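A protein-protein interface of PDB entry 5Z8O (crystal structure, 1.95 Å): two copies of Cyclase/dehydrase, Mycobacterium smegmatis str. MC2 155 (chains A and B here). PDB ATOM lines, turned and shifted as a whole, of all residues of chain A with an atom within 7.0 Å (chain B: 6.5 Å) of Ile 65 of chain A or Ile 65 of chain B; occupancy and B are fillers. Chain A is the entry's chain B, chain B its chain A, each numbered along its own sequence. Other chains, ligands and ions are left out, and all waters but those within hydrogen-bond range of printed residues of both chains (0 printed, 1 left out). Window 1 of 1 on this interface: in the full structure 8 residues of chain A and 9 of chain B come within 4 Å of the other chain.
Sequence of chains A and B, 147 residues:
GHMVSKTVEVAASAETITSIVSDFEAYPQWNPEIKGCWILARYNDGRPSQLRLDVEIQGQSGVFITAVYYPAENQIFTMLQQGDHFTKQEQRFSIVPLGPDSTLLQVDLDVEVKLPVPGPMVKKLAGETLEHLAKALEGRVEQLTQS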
ATOM      1  N   LEU A  40     -17.973  17.157   8.284  1.00  0.00           N
ATOM      2  CA  LEU A  40     -16.532  17.343   8.148  1.00  0.00           C
ATOM      3  C   LEU A  40     -16.142  18.040   6.851  1.00  0.00           C
ATOM      4  O   LEU A  40     -15.146  18.775   6.825  1.00  0.00           O
ATOM      5  CB  LEU A  40     -15.815  15.992   8.227  1.00  0.00           C
ATOM      6  CG  LEU A  40     -15.926  15.224   9.545  1.00  0.00           C
ATOM      7  CD1 LEU A  40     -15.205  13.884   9.449  1.00  0.00           C
ATOM      8  CD2 LEU A  40     -15.365  16.054  10.697  1.00  0.00           C
ATOM      9  N   GLN A  50     -18.831  14.473   3.969  1.00  0.00           N
ATOM     10  CA  GLN A  50     -18.171  13.612   4.942  1.00  0.00           C
ATOM     11  C   GLN A  50     -18.676  13.954   6.337  1.00  0.00           C
ATOM     12  O   GLN A  50     -18.823  15.131   6.678  1.00  0.00           O
ATOM     13  CB  GLN A  50     -16.644  13.769   4.877  1.00  0.00           C
ATOM     14  CG  GLN A  50     -15.873  12.768   5.732  1.00  0.00           C
ATOM     15  CD  GLN A  50     -14.377  13.026   5.730  1.00  0.00           C
ATOM     16  OE1 GLN A  50     -13.933  14.171   5.806  1.00  0.00           O
ATOM     17  NE2 GLN A  50     -13.591  11.957   5.640  1.00  0.00           N
ATOM     18  N   LEU A  51     -18.946  12.923   7.137  1.00  0.00           N
ATOM     19  CA  LEU A  51     -19.502  13.093   8.472  1.00  0.00           C
ATOM     20  C   LEU A  51     -18.661  12.358   9.503  1.00  0.00           C
ATOM     21  O   LEU A  51     -18.039  11.336   9.206  1.00  0.00           O
ATOM     22  CB  LEU A  51     -20.944  12.567   8.571  1.00  0.00           C
ATOM     23  CG  LEU A  51     -21.990  13.035   7.566  1.00  0.00           C
ATOM     24  CD1 LEU A  51     -23.263  12.208   7.727  1.00  0.00           C
ATOM     25  CD2 LEU A  51     -22.280  14.517   7.755  1.00  0.00           C
ATOM     26  N   ARG A  52     -18.674  12.877  10.729  1.00  0.00           N
ATOM     27  CA  ARG A  52     -18.293  12.119  11.913  1.00  0.00           C
ATOM     28  C   ARG A  52     -19.547  11.807  12.719  1.00  0.00           C
ATOM     29  O   ARG A  52     -20.343  12.707  13.007  1.00  0.00           O
ATOM     30  CB  ARG A  52     -17.295  12.889  12.784  1.00  0.00           C
ATOM     31  CG  ARG A  52     -17.090  12.254  14.161  1.00  0.00           C
ATOM     32  CD  ARG A  52     -16.116  13.027  15.059  1.00  0.00           C
ATOM     33  NE  ARG A  52     -16.084  12.442  16.399  1.00  0.00           N
ATOM     34  CZ  ARG A  52     -15.110  12.626  17.287  1.00  0.00           C
ATOM     35  NH1 ARG A  52     -14.061  13.380  16.987  1.00  0.00           N
ATOM     36  NH2 ARG A  52     -15.182  12.045  18.477  1.00  0.00           N
ATOM     37  N   LEU A  53     -19.719  10.537  13.087  1.00  0.00           N
ATOM     38  CA  LEU A  53     -20.857  10.090  13.883  1.00  0.00           C
ATOM     39  C   LEU A  53     -20.329   9.433  15.149  1.00  0.00           C
ATOM     40  O   LEU A  53     -19.550   8.475  15.079  1.00  0.00           O
ATOM     41  CB  LEU A  53     -21.736   9.117  13.094  1.00  0.00           C
ATOM     42  CG  LEU A  53     -23.010   8.633  13.789  1.00  0.00           C
ATOM     43  CD1 LEU A  53     -24.133   9.639  13.597  1.00  0.00           C
ATOM     44  CD2 LEU A  53     -23.421   7.253  13.286  1.00  0.00           C
ATOM     45  N   VAL A  63     -17.012   5.734  17.127  1.00  0.00           N
ATOM     46  CA  VAL A  63     -16.859   6.856  16.207  1.00  0.00           C
ATOM     47  C   VAL A  63     -16.814   6.326  14.784  1.00  0.00           C
ATOM     48  O   VAL A  63     -16.060   5.392  14.487  1.00  0.00           O
ATOM     49  CB  VAL A  63     -15.595   7.681  16.522  1.00  0.00           C
ATOM     50  CG1 VAL A  63     -15.388   8.758  15.473  1.00  0.00           C
ATOM     51  CG2 VAL A  63     -15.707   8.302  17.904  1.00  0.00           C
ATOM     52  N   PHE A  64     -17.635   6.906  13.915  1.00  0.00           N
ATOM     53  CA  PHE A  64     -17.714   6.509  12.518  1.00  0.00           C
ATOM     54  C   PHE A  64     -17.424   7.714  11.635  1.00  0.00           C
ATOM     55  O   PHE A  64     -17.994   8.791  11.845  1.00  0.00           O
ATOM     56  CB  PHE A  64     -19.096   5.925  12.238  1.00  0.00           C
ATOM     57  CG  PHE A  64     -19.419   4.758  13.118  1.00  0.00           C
ATOM     58  CD1 PHE A  64     -18.908   3.500  12.848  1.00  0.00           C
ATOM     59  CD2 PHE A  64     -20.193   4.933  14.253  1.00  0.00           C
ATOM     60  CE1 PHE A  64     -19.187   2.433  13.677  1.00  0.00           C
ATOM     61  CE2 PHE A  64     -20.476   3.870  15.087  1.00  0.00           C
ATOM     62  CZ  PHE A  64     -19.974   2.618  14.799  1.00  0.00           C
ATOM     63  N   ILE A  65     -16.547   7.531  10.650  1.00  0.00           N
ATOM     64  CA  ILE A  65     -16.263   8.545   9.641  1.00  0.00           C
ATOM     65  C   ILE A  65     -16.774   8.032   8.304  1.00  0.00           C
ATOM     66  O   ILE A  65     -16.278   7.024   7.787  1.00  0.00           O
ATOM     67  CB  ILE A  65     -14.764   8.866   9.564  1.00  0.00           C
ATOM     68  CG1 ILE A  65     -14.222   9.200  10.957  1.00  0.00           C
ATOM     69  CG2 ILE A  65     -14.522  10.008   8.587  1.00  0.00           C
ATOM     70  CD1 ILE A  65     -12.892   8.561  11.250  1.00  0.00           C
ATOM     71  N   THR A  66     -17.756   8.731   7.737  1.00  0.00           N
ATOM     72  CA  THR A  66     -18.510   8.226   6.597  1.00  0.00           C
ATOM     73  C   THR A  66     -18.551   9.264   5.486  1.00  0.00           C
ATOM     74  O   THR A  66     -18.679  10.463   5.747  1.00  0.00           O
ATOM     75  CB  THR A  66     -19.950   7.848   6.991  1.00  0.00           C
ATOM     76  OG1 THR A  66     -20.776   9.016   6.967  1.00  0.00           O
ATOM     77  CG2 THR A  66     -19.990   7.245   8.385  1.00  0.00           C
ATOM     78  N   ALA A  67     -18.442   8.793   4.248  1.00  0.00           N
ATOM     79  CA  ALA A  67     -18.640   9.634   3.081  1.00  0.00           C
ATOM     80  C   ALA A  67     -20.113   9.631   2.690  1.00  0.00           C
ATOM     81  O   ALA A  67     -20.813   8.624   2.839  1.00  0.00           O
ATOM     82  CB  ALA A  67     -17.785   9.153   1.908  1.00  0.00           C
ATOM     83  N   MET A  79     -21.257   5.783   2.976  1.00  0.00           N
ATOM     84  CA  MET A  79     -20.269   4.712   2.942  1.00  0.00           C
ATOM     85  C   MET A  79     -19.251   4.975   4.035  1.00  0.00           C
ATOM     86  O   MET A  79     -18.537   5.982   3.986  1.00  0.00           O
ATOM     87  CB  MET A  79     -19.573   4.634   1.579  1.00  0.00           C
ATOM     88  CG  MET A  79     -20.504   4.361   0.420  1.00  0.00           C
ATOM     89  SD  MET A  79     -19.633   4.264  -1.155  1.00  0.00           S
ATOM     90  CE  MET A  79     -18.652   2.787  -0.906  1.00  0.00           C
ATOM     91  N   LEU A  80     -19.189   4.079   5.017  1.00  0.00           N
ATOM     92  CA  LEU A  80     -18.203   4.201   6.079  1.00  0.00           C
ATOM     93  C   LEU A  80     -16.797   4.181   5.493  1.00  0.00           C
ATOM     94  O   LEU A  80     -16.457   3.309   4.692  1.00  0.00           O
ATOM     95  CB  LEU A  80     -18.369   3.064   7.087  1.00  0.00           C
ATOM     96  CG  LEU A  80     -17.402   3.090   8.274  1.00  0.00           C
ATOM     97  CD1 LEU A  80     -17.698   4.281   9.173  1.00  0.00           C
ATOM     98  CD2 LEU A  80     -17.460   1.790   9.061  1.00  0.00           C
ATOM     99  N   GLN A  81     -15.989   5.165   5.879  1.00  0.00           N
ATOM    100  CA  GLN A  81     -14.585   5.187   5.492  1.00  0.00           C
ATOM    101  C   GLN A  81     -13.714   4.517   6.544  1.00  0.00           C
ATOM    102  O   GLN A  81     -12.793   3.769   6.203  1.00  0.00           O
ATOM    103  CB  GLN A  81     -14.123   6.627   5.263  1.00  0.00           C
ATOM    104  CG  GLN A  81     -14.800   7.302   4.082  1.00  0.00           C
ATOM    105  CD  GLN A  81     -14.534   8.785   4.036  1.00  0.00           C
ATOM    106  OE1 GLN A  81     -14.576   9.463   5.061  1.00  0.00           O
ATOM    107  NE2 GLN A  81     -14.269   9.305   2.843  1.00  0.00           N
ATOM    108  N   GLN A  82     -13.983   4.791   7.819  1.00  0.00           N
ATOM    109  CA  GLN A  82     -13.292   4.132   8.920  1.00  0.00           C
ATOM    110  C   GLN A  82     -14.172   4.273  10.150  1.00  0.00           C
ATOM    111  O   GLN A  82     -14.706   5.355  10.406  1.00  0.00           O
ATOM    112  CB  GLN A  82     -11.900   4.741   9.167  1.00  0.00           C
ATOM    113  CG  GLN A  82     -11.025   3.990  10.187  1.00  0.00           C
ATOM    114  CD  GLN A  82     -11.477   4.138  11.634  1.00  0.00           C
ATOM    115  OE1 GLN A  82     -12.145   5.104  11.996  1.00  0.00           O
ATOM    116  NE2 GLN A  82     -11.128   3.161  12.464  1.00  0.00           N
ATOM    117  N   GLY A  83     -14.348   3.184  10.884  1.00  0.00           N
ATOM    118  CA  GLY A  83     -15.142   3.239  12.094  1.00  0.00           C
ATOM    119  C   GLY A  83     -14.758   2.125  13.035  1.00  0.00           C
ATOM    120  O   GLY A  83     -14.109   1.149  12.646  1.00  0.00           O
ATOM    121  N   ASP A  84     -15.156   2.289  14.293  1.00  0.00           N
ATOM    122  CA  ASP A  84     -15.005   1.208  15.252  1.00  0.00           C
ATOM    123  C   ASP A  84     -15.912   0.049  14.858  1.00  0.00           C
ATOM    124  O   ASP A  84     -17.029   0.256  14.375  1.00  0.00           O
ATOM    125  CB  ASP A  84     -15.342   1.683  16.668  1.00  0.00           C
ATOM    126  CG  ASP A  84     -14.369   2.727  17.182  1.00  0.00           C
ATOM    127  OD1 ASP A  84     -13.208   2.364  17.477  1.00  0.00           O
ATOM    128  OD2 ASP A  84     -14.768   3.906  17.308  1.00  0.00           O
ATOM    129  N   LEU B  40      -7.116   8.571   6.873  1.00  0.00           N
ATOM    130  CA  LEU B  40      -8.448   8.642   6.287  1.00  0.00           C
ATOM    131  C   LEU B  40      -8.422   9.066   4.826  1.00  0.00           C
ATOM    132  O   LEU B  40      -9.291   8.651   4.051  1.00  0.00           O
ATOM    133  CB  LEU B  40      -9.314   9.619   7.085  1.00  0.00           C
ATOM    134  CG  LEU B  40      -9.565   9.235   8.542  1.00  0.00           C
ATOM    135  CD1 LEU B  40     -10.378  10.311   9.244  1.00  0.00           C
ATOM    136  CD2 LEU B  40     -10.279   7.890   8.613  1.00  0.00           C
ATOM    137  N   GLN B  50      -5.613  13.430   5.841  1.00  0.00           N
ATOM    138  CA  GLN B  50      -6.602  13.446   6.908  1.00  0.00           C
ATOM    139  C   GLN B  50      -6.403  12.211   7.771  1.00  0.00           C
ATOM    140  O   GLN B  50      -6.201  11.109   7.254  1.00  0.00           O
ATOM    141  CB  GLN B  50      -8.028  13.488   6.346  1.00  0.00           C
ATOM    142  CG  GLN B  50      -9.104  13.677   7.404  1.00  0.00           C
ATOM    143  CD  GLN B  50     -10.503  13.586   6.828  1.00  0.00           C
ATOM    144  OE1 GLN B  50     -10.783  12.733   5.985  1.00  0.00           O
ATOM    145  NE2 GLN B  50     -11.391  14.464   7.283  1.00  0.00           N
ATOM    146  N   LEU B  51      -6.468  12.401   9.084  1.00  0.00           N
ATOM    147  CA  LEU B  51      -6.195  11.341  10.039  1.00  0.00           C
ATOM    148  C   LEU B  51      -7.346  11.204  11.022  1.00  0.00           C
ATOM    149  O   LEU B  51      -8.065  12.166  11.301  1.00  0.00           O
ATOM    150  CB  LEU B  51      -4.919  11.620  10.844  1.00  0.00           C
ATOM    151  CG  LEU B  51      -3.614  11.957  10.127  1.00  0.00           C
ATOM    152  CD1 LEU B  51      -2.589  12.420  11.152  1.00  0.00           C
ATOM    153  CD2 LEU B  51      -3.098  10.751   9.356  1.00  0.00           C
ATOM    154  N   ARG B  52      -7.510   9.992  11.540  1.00  0.00           N
ATOM    155  CA  ARG B  52      -8.209   9.762  12.795  1.00  0.00           C
ATOM    156  C   ARG B  52      -7.174   9.387  13.841  1.00  0.00           C
ATOM    157  O   ARG B  52      -6.339   8.508  13.603  1.00  0.00           O
ATOM    158  CB  ARG B  52      -9.254   8.652  12.689  1.00  0.00           C
ATOM    159  CG  ARG B  52      -9.771   8.235  14.068  1.00  0.00           C
ATOM    160  CD  ARG B  52     -10.784   7.111  14.011  1.00  0.00           C
ATOM    161  NE  ARG B  52     -11.139   6.661  15.355  1.00  0.00           N
ATOM    162  CZ  ARG B  52     -12.232   5.960  15.645  1.00  0.00           C
ATOM    163  NH1 ARG B  52     -13.081   5.630  14.683  1.00  0.00           N
ATOM    164  NH2 ARG B  52     -12.475   5.595  16.897  1.00  0.00           N
ATOM    165  N   LEU B  53      -7.219  10.055  14.989  1.00  0.00           N
ATOM    166  CA  LEU B  53      -6.312   9.775  16.093  1.00  0.00           C
ATOM    167  C   LEU B  53      -7.134   9.428  17.323  1.00  0.00           C
ATOM    168  O   LEU B  53      -7.979  10.222  17.748  1.00  0.00           O
ATOM    169  CB  LEU B  53      -5.398  10.968  16.390  1.00  0.00           C
ATOM    170  CG  LEU B  53      -4.437  11.419  15.291  1.00  0.00           C
ATOM    171  CD1 LEU B  53      -4.820  12.804  14.781  1.00  0.00           C
ATOM    172  CD2 LEU B  53      -3.003  11.403  15.800  1.00  0.00           C
ATOM    173  N   VAL B  63     -11.266  11.241  20.501  1.00  0.00           N
ATOM    174  CA  VAL B  63     -11.056  10.978  19.085  1.00  0.00           C
ATOM    175  C   VAL B  63     -10.873  12.310  18.376  1.00  0.00           C
ATOM    176  O   VAL B  63     -11.685  13.227  18.548  1.00  0.00           O
ATOM    177  CB  VAL B  63     -12.216  10.179  18.466  1.00  0.00           C
ATOM    178  CG1 VAL B  63     -12.021  10.039  16.958  1.00  0.00           C
ATOM    179  CG2 VAL B  63     -12.304   8.813  19.118  1.00  0.00           C
ATOM    180  N   PHE B  64      -9.810  12.406  17.583  1.00  0.00           N
ATOM    181  CA  PHE B  64      -9.488  13.582  16.789  1.00  0.00           C
ATOM    182  C   PHE B  64      -9.583  13.223  15.315  1.00  0.00           C
ATOM    183  O   PHE B  64      -9.080  12.178  14.890  1.00  0.00           O
ATOM    184  CB  PHE B  64      -8.073  14.113  17.058  1.00  0.00           C
ATOM    185  CG  PHE B  64      -7.845  14.668  18.441  1.00  0.00           C
ATOM    186  CD1 PHE B  64      -8.896  15.096  19.230  1.00  0.00           C
ATOM    187  CD2 PHE B  64      -6.550  14.807  18.924  1.00  0.00           C
ATOM    188  CE1 PHE B  64      -8.666  15.624  20.485  1.00  0.00           C
ATOM    189  CE2 PHE B  64      -6.309  15.333  20.184  1.00  0.00           C
ATOM    190  CZ  PHE B  64      -7.369  15.742  20.967  1.00  0.00           C
ATOM    191  N   ILE B  65     -10.235  14.085  14.544  1.00  0.00           N
ATOM    192  CA  ILE B  65     -10.235  14.013  13.088  1.00  0.00           C
ATOM    193  C   ILE B  65      -9.440  15.222  12.622  1.00  0.00           C
ATOM    194  O   ILE B  65      -9.844  16.366  12.862  1.00  0.00           O
ATOM    195  CB  ILE B  65     -11.657  14.016  12.508  1.00  0.00           C
ATOM    196  CG1 ILE B  65     -12.520  12.947  13.183  1.00  0.00           C
ATOM    197  CG2 ILE B  65     -11.618  13.807  10.994  1.00  0.00           C
ATOM    198  CD1 ILE B  65     -11.976  11.538  13.063  1.00  0.00           C
ATOM    199  N   THR B  66      -8.304  14.977  11.978  1.00  0.00           N
ATOM    200  CA  THR B  66      -7.310  16.021  11.778  1.00  0.00           C
ATOM    201  C   THR B  66      -6.871  16.091  10.324  1.00  0.00           C
ATOM    202  O   THR B  66      -6.653  15.061   9.682  1.00  0.00           O
ATOM    203  CB  THR B  66      -6.096  15.762  12.689  1.00  0.00           C
ATOM    204  OG1 THR B  66      -6.508  15.825  14.060  1.00  0.00           O
ATOM    205  CG2 THR B  66      -4.999  16.776  12.448  1.00  0.00           C
ATOM    206  N   ALA B  67      -6.722  17.316   9.819  1.00  0.00           N
ATOM    207  CA  ALA B  67      -6.146  17.563   8.507  1.00  0.00           C
ATOM    208  C   ALA B  67      -4.637  17.746   8.616  1.00  0.00           C
ATOM    209  O   ALA B  67      -4.127  18.291   9.599  1.00  0.00           O
ATOM    210  CB  ALA B  67      -6.770  18.800   7.862  1.00  0.00           C
ATOM    211  N   MET B  79      -4.114  20.198  11.667  1.00  0.00           N
ATOM    212  CA  MET B  79      -5.215  21.047  12.107  1.00  0.00           C
ATOM    213  C   MET B  79      -6.402  20.172  12.476  1.00  0.00           C
ATOM    214  O   MET B  79      -6.967  19.500  11.610  1.00  0.00           O
ATOM    215  CB  MET B  79      -5.603  22.044  11.012  1.00  0.00           C
ATOM    216  CG  MET B  79      -6.739  22.974  11.386  1.00  0.00           C
ATOM    217  SD  MET B  79      -7.363  23.880   9.961  1.00  0.00           S
ATOM    218  CE  MET B  79      -7.995  22.536   8.959  1.00  0.00           C
ATOM    219  N   LEU B  80      -6.780  20.184  13.753  1.00  0.00           N
ATOM    220  CA  LEU B  80      -7.961  19.448  14.181  1.00  0.00           C
ATOM    221  C   LEU B  80      -9.184  19.958  13.429  1.00  0.00           C
ATOM    222  O   LEU B  80      -9.419  21.167  13.354  1.00  0.00           O
ATOM    223  CB  LEU B  80      -8.163  19.594  15.691  1.00  0.00           C
ATOM    224  CG  LEU B  80      -9.376  18.866  16.279  1.00  0.00           C
ATOM    225  CD1 LEU B  80      -9.200  17.360  16.173  1.00  0.00           C
ATOM    226  CD2 LEU B  80      -9.606  19.275  17.721  1.00  0.00           C
ATOM    227  N   GLN B  81      -9.938  19.034  12.830  1.00  0.00           N
ATOM    228  CA  GLN B  81     -11.190  19.362  12.159  1.00  0.00           C
ATOM    229  C   GLN B  81     -12.393  19.197  13.078  1.00  0.00           C
ATOM    230  O   GLN B  81     -13.285  20.048  13.096  1.00  0.00           O
ATOM    231  CB  GLN B  81     -11.365  18.482  10.917  1.00  0.00           C
ATOM    232  CG  GLN B  81     -10.362  18.755   9.809  1.00  0.00           C
ATOM    233  CD  GLN B  81     -10.388  17.690   8.726  1.00  0.00           C
ATOM    234  OE1 GLN B  81     -10.440  16.496   9.016  1.00  0.00           O
ATOM    235  NE2 GLN B  81     -10.362  18.121   7.470  1.00  0.00           N
ATOM    236  N   GLN B  82     -12.425  18.105  13.835  1.00  0.00           N
ATOM    237  CA  GLN B  82     -13.456  17.851  14.831  1.00  0.00           C
ATOM    238  C   GLN B  82     -12.879  16.869  15.832  1.00  0.00           C
ATOM    239  O   GLN B  82     -12.388  15.805  15.442  1.00  0.00           O
ATOM    240  CB  GLN B  82     -14.730  17.283  14.183  1.00  0.00           C
ATOM    241  CG  GLN B  82     -15.897  17.044  15.146  1.00  0.00           C
ATOM    242  CD  GLN B  82     -16.345  18.295  15.879  1.00  0.00           C
ATOM    243  OE1 GLN B  82     -16.513  19.356  15.278  1.00  0.00           O
ATOM    244  NE2 GLN B  82     -16.540  18.176  17.191  1.00  0.00           N
ATOM    245  N   GLY B  83     -12.970  17.201  17.112  1.00  0.00           N
ATOM    246  CA  GLY B  83     -12.434  16.309  18.119  1.00  0.00           C
ATOM    247  C   GLY B  83     -13.094  16.522  19.458  1.00  0.00           C
ATOM    248  O   GLY B  83     -13.749  17.540  19.701  1.00  0.00           O
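Among the printed residues, pairs that only touch across the chains: Leu 40 of chain A with Ile 65 of chain B (3.9 Å), Leu 40 of chain A with Gln 82 of chain B (3.8 Å), Arg 52 of chain A with Gly 83 of chain B (3.5 Å), Val 63 of chain A with Val 63 of chain B (3.6 Å), Ile 65 of chain A with Leu 40 of chain B (3.7 Å), Ile 65 of chain A with Arg 52 of chain B (3.8 Å), Ile 65 of chain A with Ile 65 of chain B (3.6 Å) and Gln 82 of chain A with Leu 40 of chain B (3.6 Å).
Of the 15 printed residues of chain B, 7 touch a printed residue of chain A.
Among the printed residues, 14 pairs touch across the chains.
Ile 65 of chain A touches just these residues of chain B: Leu 40, Arg 52 and Ile 65.
Ile 65 of chain B touches just these residues of chain A: Leu 40 (3.9 Å) and Ile 65 (3.6 Å).
Of the printed residues of chain A, Arg 52 of chain B touches Val 63, Ile 65, Gln 82 and Asp 84.
Of the printed residues of chain A, Val 63 of chain B touches Arg 52 (2.8 Å) and Val 63 (3.6 Å).
Printed residues of chain B within 4 Å of Gln 82 of chain A: Leu 40 (3.6 Å) and Arg 52 (2.9 Å).
Of the printed residues of chain A, Gly 83 of chain B touches Arg 52.
Of the printed residues of chain B, Asp 84 of chain A touches Arg 52 (2.9 Å).
Met 79 of chain B touches none of the printed residues of chain A.
Met 79 of chain A touches none of the printed residues of chain B.
The nearest residue of chain B that does not touch Ile 65 of chain A is Gln 50 of chain B (5.3 Å).
The nearest residue of chain A that does not touch Ile 65 of chain B is Arg 52 of chain A (4.1 Å).
The nearest printed residue of chain A that does not touch Arg 52 of chain B is Gly 83 of chain A (4.1 Å).
Leu 40 of chain A touches Ile 65 of chain B, and with the chains exchanged Ile 65 of chain A touches Leu 40 of chain B.
Leu 40 of chain A touches Gln 82 of chain B, and with the chains exchanged Gln 82 of chain A touches Leu 40 of chain B.
Arg 52 of chain A touches Val 63 of chain B, and with the chains exchanged Val 63 of chain A touches Arg 52 of chain B.
Arg 52 of chain A touches Gly 83 of chain B, but with the chains exchanged Gly 83 of chain A does not touch Arg 52 of chain B (4.1 Å).
Positions printed for both chains: 40, 50, 51, 52, 53, 63, 64, 65, 66, 67, 79, 80, 81, 82 and 83.
NH1 of Arg 52 of chain B lies within hydrogen-bond range of O of Val 63 of chain A (3.0 Å).
The side-chain amide oxygen (OE1) of Gln 82 of chain A is in hydrogen-bond range of the guanidinium group (NH1) of Arg 52 of chain B (2.9 Å).
OE1 of Gln 50 of chain B sits at hydrogen-bond distance from NE2 of Gln 50 of chain A, 2.9 Å away.
O of Val 63 of chain B lies within hydrogen-bond range of NH1 of Arg 52 of chain A (2.8 Å).
The side-chain carboxylate (OD2) of Asp 84 of chain A lies within salt-bridge range of the guanidinium group (NH2) of Arg 52 of chain B.
NH1 of Arg 52 of chain A is in hydrogen-bond range of O of Gln 82 of chain B (3.3 Å).
The backbone carbonyl oxygen (O) of Gln 82 of chain B is in hydrogen-bond range of the backbone NH (N) of Ile 65 of chain B, at 2.9 Å.
O of Ile 65 of chain B sits at hydrogen-bond distance from N of Gln 81 of chain B (2.7 Å).
The backbone carbonyl oxygen of Gln 50 of chain B is in hydrogen-bond range of the backbone NH of Leu 40 of chain B.
The backbone NH (N) of Gln 81 of chain A is in hydrogen-bond range of the backbone carbonyl oxygen (O) of Ile 65 of chain A, at 2.7 Å.
NE2 of Gln 50 of chain B is in hydrogen-bond range of OE1 of Gln 81 of chain B (2.8 Å).
NE2 of Gln 50 of chain A is in hydrogen-bond range of OE1 of Gln 81 of chain A (2.7 Å).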
